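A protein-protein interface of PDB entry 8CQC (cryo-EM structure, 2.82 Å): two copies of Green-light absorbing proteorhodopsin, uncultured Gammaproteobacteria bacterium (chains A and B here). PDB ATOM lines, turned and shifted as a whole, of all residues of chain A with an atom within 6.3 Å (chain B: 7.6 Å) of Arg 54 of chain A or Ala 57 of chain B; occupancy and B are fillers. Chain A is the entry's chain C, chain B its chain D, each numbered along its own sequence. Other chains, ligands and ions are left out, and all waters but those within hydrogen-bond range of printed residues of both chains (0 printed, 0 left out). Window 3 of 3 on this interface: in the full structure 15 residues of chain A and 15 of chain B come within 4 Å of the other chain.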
ATOM      1  N   VAL A  50       8.104   5.108   6.171  1.00  0.00           N
ATOM      2  CA  VAL A  50       7.101   4.477   5.322  1.00  0.00           C
ATOM      3  C   VAL A  50       6.876   3.023   5.722  1.00  0.00           C
ATOM      4  O   VAL A  50       5.745   2.529   5.685  1.00  0.00           O
ATOM      5  CB  VAL A  50       7.522   4.617   3.847  1.00  0.00           C
ATOM      6  CG1 VAL A  50       6.915   3.530   3.003  1.00  0.00           C
ATOM      7  CG2 VAL A  50       7.111   5.975   3.316  1.00  0.00           C
ATOM      8  N   GLU A  51       7.930   2.322   6.137  1.00  0.00           N
ATOM      9  CA  GLU A  51       7.846   0.901   6.439  1.00  0.00           C
ATOM     10  C   GLU A  51       7.238   0.600   7.799  1.00  0.00           C
ATOM     11  O   GLU A  51       7.282  -0.555   8.230  1.00  0.00           O
ATOM     12  CB  GLU A  51       9.234   0.268   6.344  1.00  0.00           C
ATOM     13  CG  GLU A  51       9.735   0.087   4.924  1.00  0.00           C
ATOM     14  CD  GLU A  51       8.938  -0.937   4.148  1.00  0.00           C
ATOM     15  OE1 GLU A  51       7.872  -0.587   3.606  1.00  0.00           O
ATOM     16  OE2 GLU A  51       9.374  -2.101   4.086  1.00  0.00           O
ATOM     17  N   ARG A  52       6.678   1.594   8.488  1.00  0.00           N
ATOM     18  CA  ARG A  52       5.966   1.325   9.730  1.00  0.00           C
ATOM     19  C   ARG A  52       4.645   0.607   9.500  1.00  0.00           C
ATOM     20  O   ARG A  52       4.037   0.142  10.468  1.00  0.00           O
ATOM     21  CB  ARG A  52       5.725   2.629  10.488  1.00  0.00           C
ATOM     22  CG  ARG A  52       6.992   3.303  10.968  1.00  0.00           C
ATOM     23  CD  ARG A  52       6.726   4.703  11.490  1.00  0.00           C
ATOM     24  NE  ARG A  52       6.008   4.709  12.758  1.00  0.00           N
ATOM     25  CZ  ARG A  52       4.708   4.930  12.886  1.00  0.00           C
ATOM     26  NH1 ARG A  52       3.940   5.154  11.835  1.00  0.00           N
ATOM     27  NH2 ARG A  52       4.166   4.934  14.100  1.00  0.00           N
ATOM     28  N   ASP A  53       4.186   0.515   8.251  1.00  0.00           N
ATOM     29  CA  ASP A  53       2.964  -0.225   7.957  1.00  0.00           C
ATOM     30  C   ASP A  53       3.173  -1.727   8.077  1.00  0.00           C
ATOM     31  O   ASP A  53       2.218  -2.463   8.349  1.00  0.00           O
ATOM     32  CB  ASP A  53       2.466   0.121   6.556  1.00  0.00           C
ATOM     33  CG  ASP A  53       2.300   1.607   6.349  1.00  0.00           C
ATOM     34  OD1 ASP A  53       2.762   2.381   7.213  1.00  0.00           O
ATOM     35  OD2 ASP A  53       1.706   2.001   5.325  1.00  0.00           O
ATOM     36  N   ARG A  54       4.400  -2.200   7.874  1.00  0.00           N
ATOM     37  CA  ARG A  54       4.685  -3.626   7.915  1.00  0.00           C
ATOM     38  C   ARG A  54       4.923  -4.155   9.321  1.00  0.00           C
ATOM     39  O   ARG A  54       5.066  -5.370   9.488  1.00  0.00           O
ATOM     40  CB  ARG A  54       5.906  -3.947   7.055  1.00  0.00           C
ATOM     41  CG  ARG A  54       5.765  -3.592   5.596  1.00  0.00           C
ATOM     42  CD  ARG A  54       6.802  -4.336   4.791  1.00  0.00           C
ATOM     43  NE  ARG A  54       6.644  -5.775   4.945  1.00  0.00           N
ATOM     44  CZ  ARG A  54       7.560  -6.672   4.612  1.00  0.00           C
ATOM     45  NH1 ARG A  54       8.730  -6.313   4.117  1.00  0.00           N
ATOM     46  NH2 ARG A  54       7.298  -7.962   4.790  1.00  0.00           N
ATOM     47  N   VAL A  55       4.973  -3.291  10.329  1.00  0.00           N
ATOM     48  CA  VAL A  55       5.300  -3.707  11.684  1.00  0.00           C
ATOM     49  C   VAL A  55       4.078  -3.535  12.575  1.00  0.00           C
ATOM     50  O   VAL A  55       3.154  -2.772  12.279  1.00  0.00           O
ATOM     51  CB  VAL A  55       6.510  -2.935  12.251  1.00  0.00           C
ATOM     52  CG1 VAL A  55       7.699  -3.065  11.322  1.00  0.00           C
ATOM     53  CG2 VAL A  55       6.159  -1.478  12.474  1.00  0.00           C
ATOM     54  N   SER A  56       4.078  -4.270  13.683  1.00  0.00           N
ATOM     55  CA  SER A  56       3.007  -4.169  14.657  1.00  0.00           C
ATOM     56  C   SER A  56       3.098  -2.838  15.403  1.00  0.00           C
ATOM     57  O   SER A  56       4.059  -2.080  15.263  1.00  0.00           O
ATOM     58  CB  SER A  56       3.065  -5.340  15.636  1.00  0.00           C
ATOM     59  OG  SER A  56       2.014  -5.263  16.580  1.00  0.00           O
ATOM     60  N   LEU A  63      10.758   2.055  14.769  1.00  0.00           N
ATOM     61  CA  LEU A  63      10.956   2.526  13.401  1.00  0.00           C
ATOM     62  C   LEU A  63      10.875   4.047  13.317  1.00  0.00           C
ATOM     63  O   LEU A  63      11.620   4.676  12.555  1.00  0.00           O
ATOM     64  CB  LEU A  63       9.948   1.869  12.461  1.00  0.00           C
ATOM     65  CG  LEU A  63      10.485   0.646  11.712  1.00  0.00           C
ATOM     66  CD1 LEU A  63      10.820  -0.480  12.670  1.00  0.00           C
ATOM     67  CD2 LEU A  63       9.497   0.179  10.666  1.00  0.00           C
ATOM     68  N   TRP A 240      14.639  -2.501  11.652  1.00  0.00           N
ATOM     69  CA  TRP A 240      13.528  -2.725  10.733  1.00  0.00           C
ATOM     70  C   TRP A 240      13.380  -4.199  10.395  1.00  0.00           C
ATOM     71  O   TRP A 240      12.262  -4.719  10.328  1.00  0.00           O
ATOM     72  CB  TRP A 240      13.735  -1.905   9.457  1.00  0.00           C
ATOM     73  CG  TRP A 240      12.871  -2.341   8.314  1.00  0.00           C
ATOM     74  CD1 TRP A 240      11.595  -1.942   8.052  1.00  0.00           C
ATOM     75  CD2 TRP A 240      13.222  -3.265   7.278  1.00  0.00           C
ATOM     76  NE1 TRP A 240      11.129  -2.562   6.921  1.00  0.00           N
ATOM     77  CE2 TRP A 240      12.110  -3.379   6.427  1.00  0.00           C
ATOM     78  CE3 TRP A 240      14.370  -4.008   6.990  1.00  0.00           C
ATOM     79  CZ2 TRP A 240      12.112  -4.202   5.308  1.00  0.00           C
ATOM     80  CZ3 TRP A 240      14.367  -4.824   5.882  1.00  0.00           C
ATOM     81  CH2 TRP A 240      13.247  -4.916   5.054  1.00  0.00           C
ATOM     82  N   ALA A 243      11.929  -6.051  13.409  1.00  0.00           N
ATOM     83  CA  ALA A 243      10.543  -5.651  13.622  1.00  0.00           C
ATOM     84  C   ALA A 243       9.616  -6.278  12.590  1.00  0.00           C
ATOM     85  O   ALA A 243       8.549  -6.796  12.940  1.00  0.00           O
ATOM     86  CB  ALA A 243      10.431  -4.129  13.588  1.00  0.00           C
ATOM     87  N   VAL A 244      10.005  -6.242  11.313  1.00  0.00           N
ATOM     88  CA  VAL A 244       9.181  -6.830  10.261  1.00  0.00           C
ATOM     89  C   VAL A 244       9.088  -8.338  10.438  1.00  0.00           C
ATOM     90  O   VAL A 244       8.015  -8.932  10.269  1.00  0.00           O
ATOM     91  CB  VAL A 244       9.736  -6.445   8.876  1.00  0.00           C
ATOM     92  CG1 VAL A 244       9.141  -7.324   7.801  1.00  0.00           C
ATOM     93  CG2 VAL A 244       9.438  -4.987   8.582  1.00  0.00           C
ATOM     94  N   SER A 247       6.690  -9.004  13.362  1.00  0.00           N
ATOM     95  CA  SER A 247       5.309  -8.653  13.053  1.00  0.00           C
ATOM     96  C   SER A 247       4.685  -9.631  12.067  1.00  0.00           C
ATOM     97  O   SER A 247       3.509  -9.985  12.201  1.00  0.00           O
ATOM     98  CB  SER A 247       5.243  -7.226  12.519  1.00  0.00           C
ATOM     99  OG  SER A 247       5.631  -6.307  13.521  1.00  0.00           O
ATOM    100  N   SER A 248       5.444 -10.071  11.060  1.00  0.00           N
ATOM    101  CA  SER A 248       4.919 -11.077  10.143  1.00  0.00           C
ATOM    102  C   SER A 248       4.751 -12.416  10.847  1.00  0.00           C
ATOM    103  O   SER A 248       3.736 -13.100  10.670  1.00  0.00           O
ATOM    104  CB  SER A 248       5.836 -11.220   8.929  1.00  0.00           C
ATOM    105  OG  SER A 248       7.021 -11.917   9.263  1.00  0.00           O
ATOM    106  N   ARG B  52       1.027   1.881  -2.267  1.00  0.00           N
ATOM    107  CA  ARG B  52       1.278   0.803  -1.320  1.00  0.00           C
ATOM    108  C   ARG B  52       0.022   0.376  -0.576  1.00  0.00           C
ATOM    109  O   ARG B  52       0.048  -0.645   0.116  1.00  0.00           O
ATOM    110  CB  ARG B  52       2.355   1.222  -0.321  1.00  0.00           C
ATOM    111  CG  ARG B  52       3.713   1.455  -0.940  1.00  0.00           C
ATOM    112  CD  ARG B  52       4.671   2.112   0.039  1.00  0.00           C
ATOM    113  NE  ARG B  52       5.060   1.225   1.127  1.00  0.00           N
ATOM    114  CZ  ARG B  52       4.529   1.247   2.341  1.00  0.00           C
ATOM    115  NH1 ARG B  52       3.568   2.096   2.660  1.00  0.00           N
ATOM    116  NH2 ARG B  52       4.979   0.399   3.260  1.00  0.00           N
ATOM    117  N   VAL B  55      -1.520  -2.995  -2.102  1.00  0.00           N
ATOM    118  CA  VAL B  55      -0.738  -4.218  -2.027  1.00  0.00           C
ATOM    119  C   VAL B  55      -0.737  -4.731  -0.594  1.00  0.00           C
ATOM    120  O   VAL B  55      -0.961  -3.990   0.367  1.00  0.00           O
ATOM    121  CB  VAL B  55       0.704  -4.017  -2.541  1.00  0.00           C
ATOM    122  CG1 VAL B  55       0.689  -3.481  -3.958  1.00  0.00           C
ATOM    123  CG2 VAL B  55       1.476  -3.090  -1.625  1.00  0.00           C
ATOM    124  N   SER B  56      -0.486  -6.029  -0.459  1.00  0.00           N
ATOM    125  CA  SER B  56      -0.396  -6.650   0.851  1.00  0.00           C
ATOM    126  C   SER B  56       0.881  -6.203   1.558  1.00  0.00           C
ATOM    127  O   SER B  56       1.735  -5.524   0.988  1.00  0.00           O
ATOM    128  CB  SER B  56      -0.436  -8.171   0.722  1.00  0.00           C
ATOM    129  OG  SER B  56      -0.347  -8.791   1.991  1.00  0.00           O
ATOM    130  N   ALA B  57       1.053  -6.603   2.783  1.00  0.00           N
ATOM    131  CA  ALA B  57       2.255  -6.229   3.528  1.00  0.00           C
ATOM    132  C   ALA B  57       3.525  -6.819   2.921  1.00  0.00           C
ATOM    133  O   ALA B  57       4.607  -6.251   3.075  1.00  0.00           O
ATOM    134  CB  ALA B  57       2.122  -6.644   4.985  1.00  0.00           C
ATOM    135  N   LYS B  58       3.415  -7.952   2.228  1.00  0.00           N
ATOM    136  CA  LYS B  58       4.599  -8.608   1.667  1.00  0.00           C
ATOM    137  C   LYS B  58       5.189  -7.844   0.494  1.00  0.00           C
ATOM    138  O   LYS B  58       6.370  -7.984   0.196  1.00  0.00           O
ATOM    139  CB  LYS B  58       4.251 -10.021   1.207  1.00  0.00           C
ATOM    140  CG  LYS B  58       3.505 -10.851   2.235  1.00  0.00           C
ATOM    141  CD  LYS B  58       3.147 -12.209   1.657  1.00  0.00           C
ATOM    142  CE  LYS B  58       2.412 -12.058   0.336  1.00  0.00           C
ATOM    143  NZ  LYS B  58       2.100 -13.377  -0.282  1.00  0.00           N
ATOM    144  N   TRP B  59       4.366  -7.028  -0.146  1.00  0.00           N
ATOM    145  CA  TRP B  59       4.810  -6.286  -1.322  1.00  0.00           C
ATOM    146  C   TRP B  59       5.109  -4.821  -1.032  1.00  0.00           C
ATOM    147  O   TRP B  59       5.654  -4.120  -1.905  1.00  0.00           O
ATOM    148  CB  TRP B  59       3.751  -6.380  -2.419  1.00  0.00           C
ATOM    149  CG  TRP B  59       3.440  -7.780  -2.824  1.00  0.00           C
ATOM    150  CD1 TRP B  59       2.466  -8.582  -2.317  1.00  0.00           C
ATOM    151  CD2 TRP B  59       4.111  -8.549  -3.826  1.00  0.00           C
ATOM    152  NE1 TRP B  59       2.489  -9.806  -2.935  1.00  0.00           N
ATOM    153  CE2 TRP B  59       3.491  -9.811  -3.869  1.00  0.00           C
ATOM    154  CE3 TRP B  59       5.180  -8.294  -4.690  1.00  0.00           C
ATOM    155  CZ2 TRP B  59       3.899 -10.813  -4.740  1.00  0.00           C
ATOM    156  CZ3 TRP B  59       5.582  -9.290  -5.555  1.00  0.00           C
ATOM    157  CH2 TRP B  59       4.945 -10.534  -5.572  1.00  0.00           C
ATOM    158  N   LYS B  60       4.764  -4.381   0.140  1.00  0.00           N
ATOM    159  CA  LYS B  60       4.962  -2.975   0.485  1.00  0.00           C
ATOM    160  C   LYS B  60       6.407  -2.533   0.299  1.00  0.00           C
ATOM    161  O   LYS B  60       6.668  -1.497  -0.310  1.00  0.00           O
ATOM    162  CB  LYS B  60       4.516  -2.717   1.925  1.00  0.00           C
ATOM    163  CG  LYS B  60       3.010  -2.745   2.107  1.00  0.00           C
ATOM    164  CD  LYS B  60       2.622  -2.572   3.564  1.00  0.00           C
ATOM    165  CE  LYS B  60       1.119  -2.407   3.705  1.00  0.00           C
ATOM    166  NZ  LYS B  60       0.373  -3.486   3.000  1.00  0.00           N
ATOM    167  N   THR B  61       7.344  -3.317   0.820  1.00  0.00           N
ATOM    168  CA  THR B  61       8.752  -2.964   0.703  1.00  0.00           C
ATOM    169  C   THR B  61       9.138  -2.837  -0.758  1.00  0.00           C
ATOM    170  O   THR B  61       9.790  -1.871  -1.152  1.00  0.00           O
ATOM    171  CB  THR B  61       9.655  -4.017   1.363  1.00  0.00           C
ATOM    172  OG1 THR B  61       9.248  -4.211   2.722  1.00  0.00           O
ATOM    173  CG2 THR B  61      11.108  -3.565   1.334  1.00  0.00           C
ATOM    174  N   SER B  62       8.733  -3.810  -1.567  1.00  0.00           N
ATOM    175  CA  SER B  62       9.033  -3.757  -2.990  1.00  0.00           C
ATOM    176  C   SER B  62       8.621  -2.406  -3.547  1.00  0.00           C
ATOM    177  O   SER B  62       9.406  -1.742  -4.224  1.00  0.00           O
ATOM    178  CB  SER B  62       8.316  -4.883  -3.735  1.00  0.00           C
ATOM    179  OG  SER B  62       8.726  -6.153  -3.260  1.00  0.00           O
ATOM    180  N   THR B  64       8.026   0.328  -1.791  1.00  0.00           N
ATOM    181  CA  THR B  64       8.788   1.366  -1.112  1.00  0.00           C
ATOM    182  C   THR B  64      10.077   1.623  -1.871  1.00  0.00           C
ATOM    183  O   THR B  64      10.421   2.771  -2.152  1.00  0.00           O
ATOM    184  CB  THR B  64       9.114   0.969   0.338  1.00  0.00           C
ATOM    185  OG1 THR B  64       7.903   0.652   1.036  1.00  0.00           O
ATOM    186  CG2 THR B  64       9.828   2.105   1.055  1.00  0.00           C
ATOM    187  N   LEU B 112      13.469  -8.913  -3.455  1.00  0.00           N
ATOM    188  CA  LEU B 112      12.259  -8.516  -2.743  1.00  0.00           C
ATOM    189  C   LEU B 112      11.024  -9.209  -3.310  1.00  0.00           C
ATOM    190  O   LEU B 112      10.176  -9.699  -2.556  1.00  0.00           O
ATOM    191  CB  LEU B 112      12.100  -7.000  -2.783  1.00  0.00           C
ATOM    192  CG  LEU B 112      13.025  -6.245  -1.832  1.00  0.00           C
ATOM    193  CD1 LEU B 112      12.774  -4.766  -1.941  1.00  0.00           C
ATOM    194  CD2 LEU B 112      12.814  -6.719  -0.409  1.00  0.00           C
ATOM    195  N   ALA B 115      11.164 -12.846  -2.313  1.00  0.00           N
ATOM    196  CA  ALA B 115      10.832 -13.047  -0.907  1.00  0.00           C
ATOM    197  C   ALA B 115       9.347 -12.845  -0.645  1.00  0.00           C
ATOM    198  O   ALA B 115       8.778 -13.510   0.227  1.00  0.00           O
ATOM    199  CB  ALA B 115      11.657 -12.107  -0.031  1.00  0.00           C
ATOM    200  N   ALA B 116       8.708 -11.934  -1.375  1.00  0.00           N
ATOM    201  CA  ALA B 116       7.274 -11.722  -1.238  1.00  0.00           C
ATOM    202  C   ALA B 116       6.446 -12.780  -1.958  1.00  0.00           C
ATOM    203  O   ALA B 116       5.245 -12.884  -1.696  1.00  0.00           O
ATOM    204  CB  ALA B 116       6.899 -10.332  -1.751  1.00  0.00           C
ATOM    205  N   SER B 247      -1.909  -9.178  -4.703  1.00  0.00           N
ATOM    206  CA  SER B 247      -2.634  -8.766  -3.506  1.00  0.00           C
ATOM    207  C   SER B 247      -4.142  -8.829  -3.713  1.00  0.00           C
ATOM    208  O   SER B 247      -4.877  -9.234  -2.807  1.00  0.00           O
ATOM    209  CB  SER B 247      -2.201  -7.363  -3.094  1.00  0.00           C
ATOM    210  OG  SER B 247      -0.823  -7.347  -2.774  1.00  0.00           O
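Of the 14 printed residues of chain B, 5 touch a printed residue of chain A.
Printed residues of chain B that touch a printed residue of chain A: Arg 52, Ala 57, Lys 60, Thr 61 and Thr 64.
Of the 13 printed residues of chain A, 5 touch a printed residue of chain B.
Printed residues of chain A that touch a printed residue of chain B: Val 50, Glu 51, Asp 53, Arg 54 and Trp 240.
Hydrophobic or aromatic side chains of chain A that line the printed part of chain B: Val 50 and Trp 240.
Along chain A the printed residues that touch a printed residue of chain B span positions 50 to 240.
Of chain B, only Ala 57 (2.8 Å), Lys 60 (3.9 Å) and Thr 61 (2.6 Å) come within 4 Å of Arg 54 of chain A.
Of the printed residues of chain A, Thr 61 of chain B touches Glu 51 (2.5 Å), Arg 54 (2.6 Å) and Trp 240 (3.9 Å).
Printed residues of chain B within 4 Å of Trp 240 of chain A: Thr 61 (3.9 Å).
Ser 247 of chain B touches none of the printed residues of chain A.
The nearest residue of chain B that does not touch Arg 54 of chain A is Lys 58 of chain B (4.2 Å).
4 positions are printed for both chains.
Of the 10 pairs that touch across the chains among the printed residues, none has its exchanged pair printed and touching as well.
The backbone carbonyl oxygen (O) of Ala 57 of chain B sits at hydrogen-bond distance from the guanidinium group (NE) of Arg 54 of chain A (2.8 Å).
OE1 of Glu 51 of chain A sits at hydrogen-bond distance from OG1 of Thr 64 of chain B, at 2.9 Å.
The side-chain carboxylate of Asp 53 of chain A is in salt-bridge range of the guanidinium group of Arg 52 of chain B.
NH2 of Arg 52 of chain B is in hydrogen-bond range of O of Val 50 of chain A (3.3 Å).
OE2 of Glu 51 of chain A lies within hydrogen-bond range of OG1 of Thr 61 of chain B, at 2.5 Å.
OG1 of Thr 61 of chain B is in hydrogen-bond range of NH1 of Arg 54 of chain A (2.6 Å).
OE1 of Glu 51 of chain A is in salt-bridge range of NH2 of Arg 52 of chain B.
Among the printed residues, merely in contact across the chains: Val 50 of chain A with Thr 64 of chain B (3.6 Å), Trp 240 of chain A with Thr 61 of chain B (3.9 Å) and Arg 54 of chain A with Lys 60 of chain B (3.9 Å).
The side-chain amino group of Lys 60 of chain B lies close to the backbone carbonyl oxygen of Ser 56 of chain B (3.2 Å).
The guanidinium group (NE) of Arg 52 of chain B lies within hydrogen-bond range of the side-chain hydroxyl (OG1) of Thr 64 of chain B (2.9 Å).
The backbone carbonyl oxygen of Lys 60 of chain B sits at hydrogen-bond distance from the guanidinium group of Arg 52 of chain B, at 3.5 Å.
The side-chain hydroxyl (OG1) of Thr 64 of chain B is in hydrogen-bond range of the backbone carbonyl oxygen (O) of Lys 60 of chain B (2.8 Å).
The side-chain carboxylate (OE2) of Glu 51 of chain A lies within hydrogen-bond range of the indole nitrogen (NE1) of Trp 240 of chain A.
NZ of Lys 60 of chain B lies within hydrogen-bond range of O of Val 55 of chain B, 3.0 Å away.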
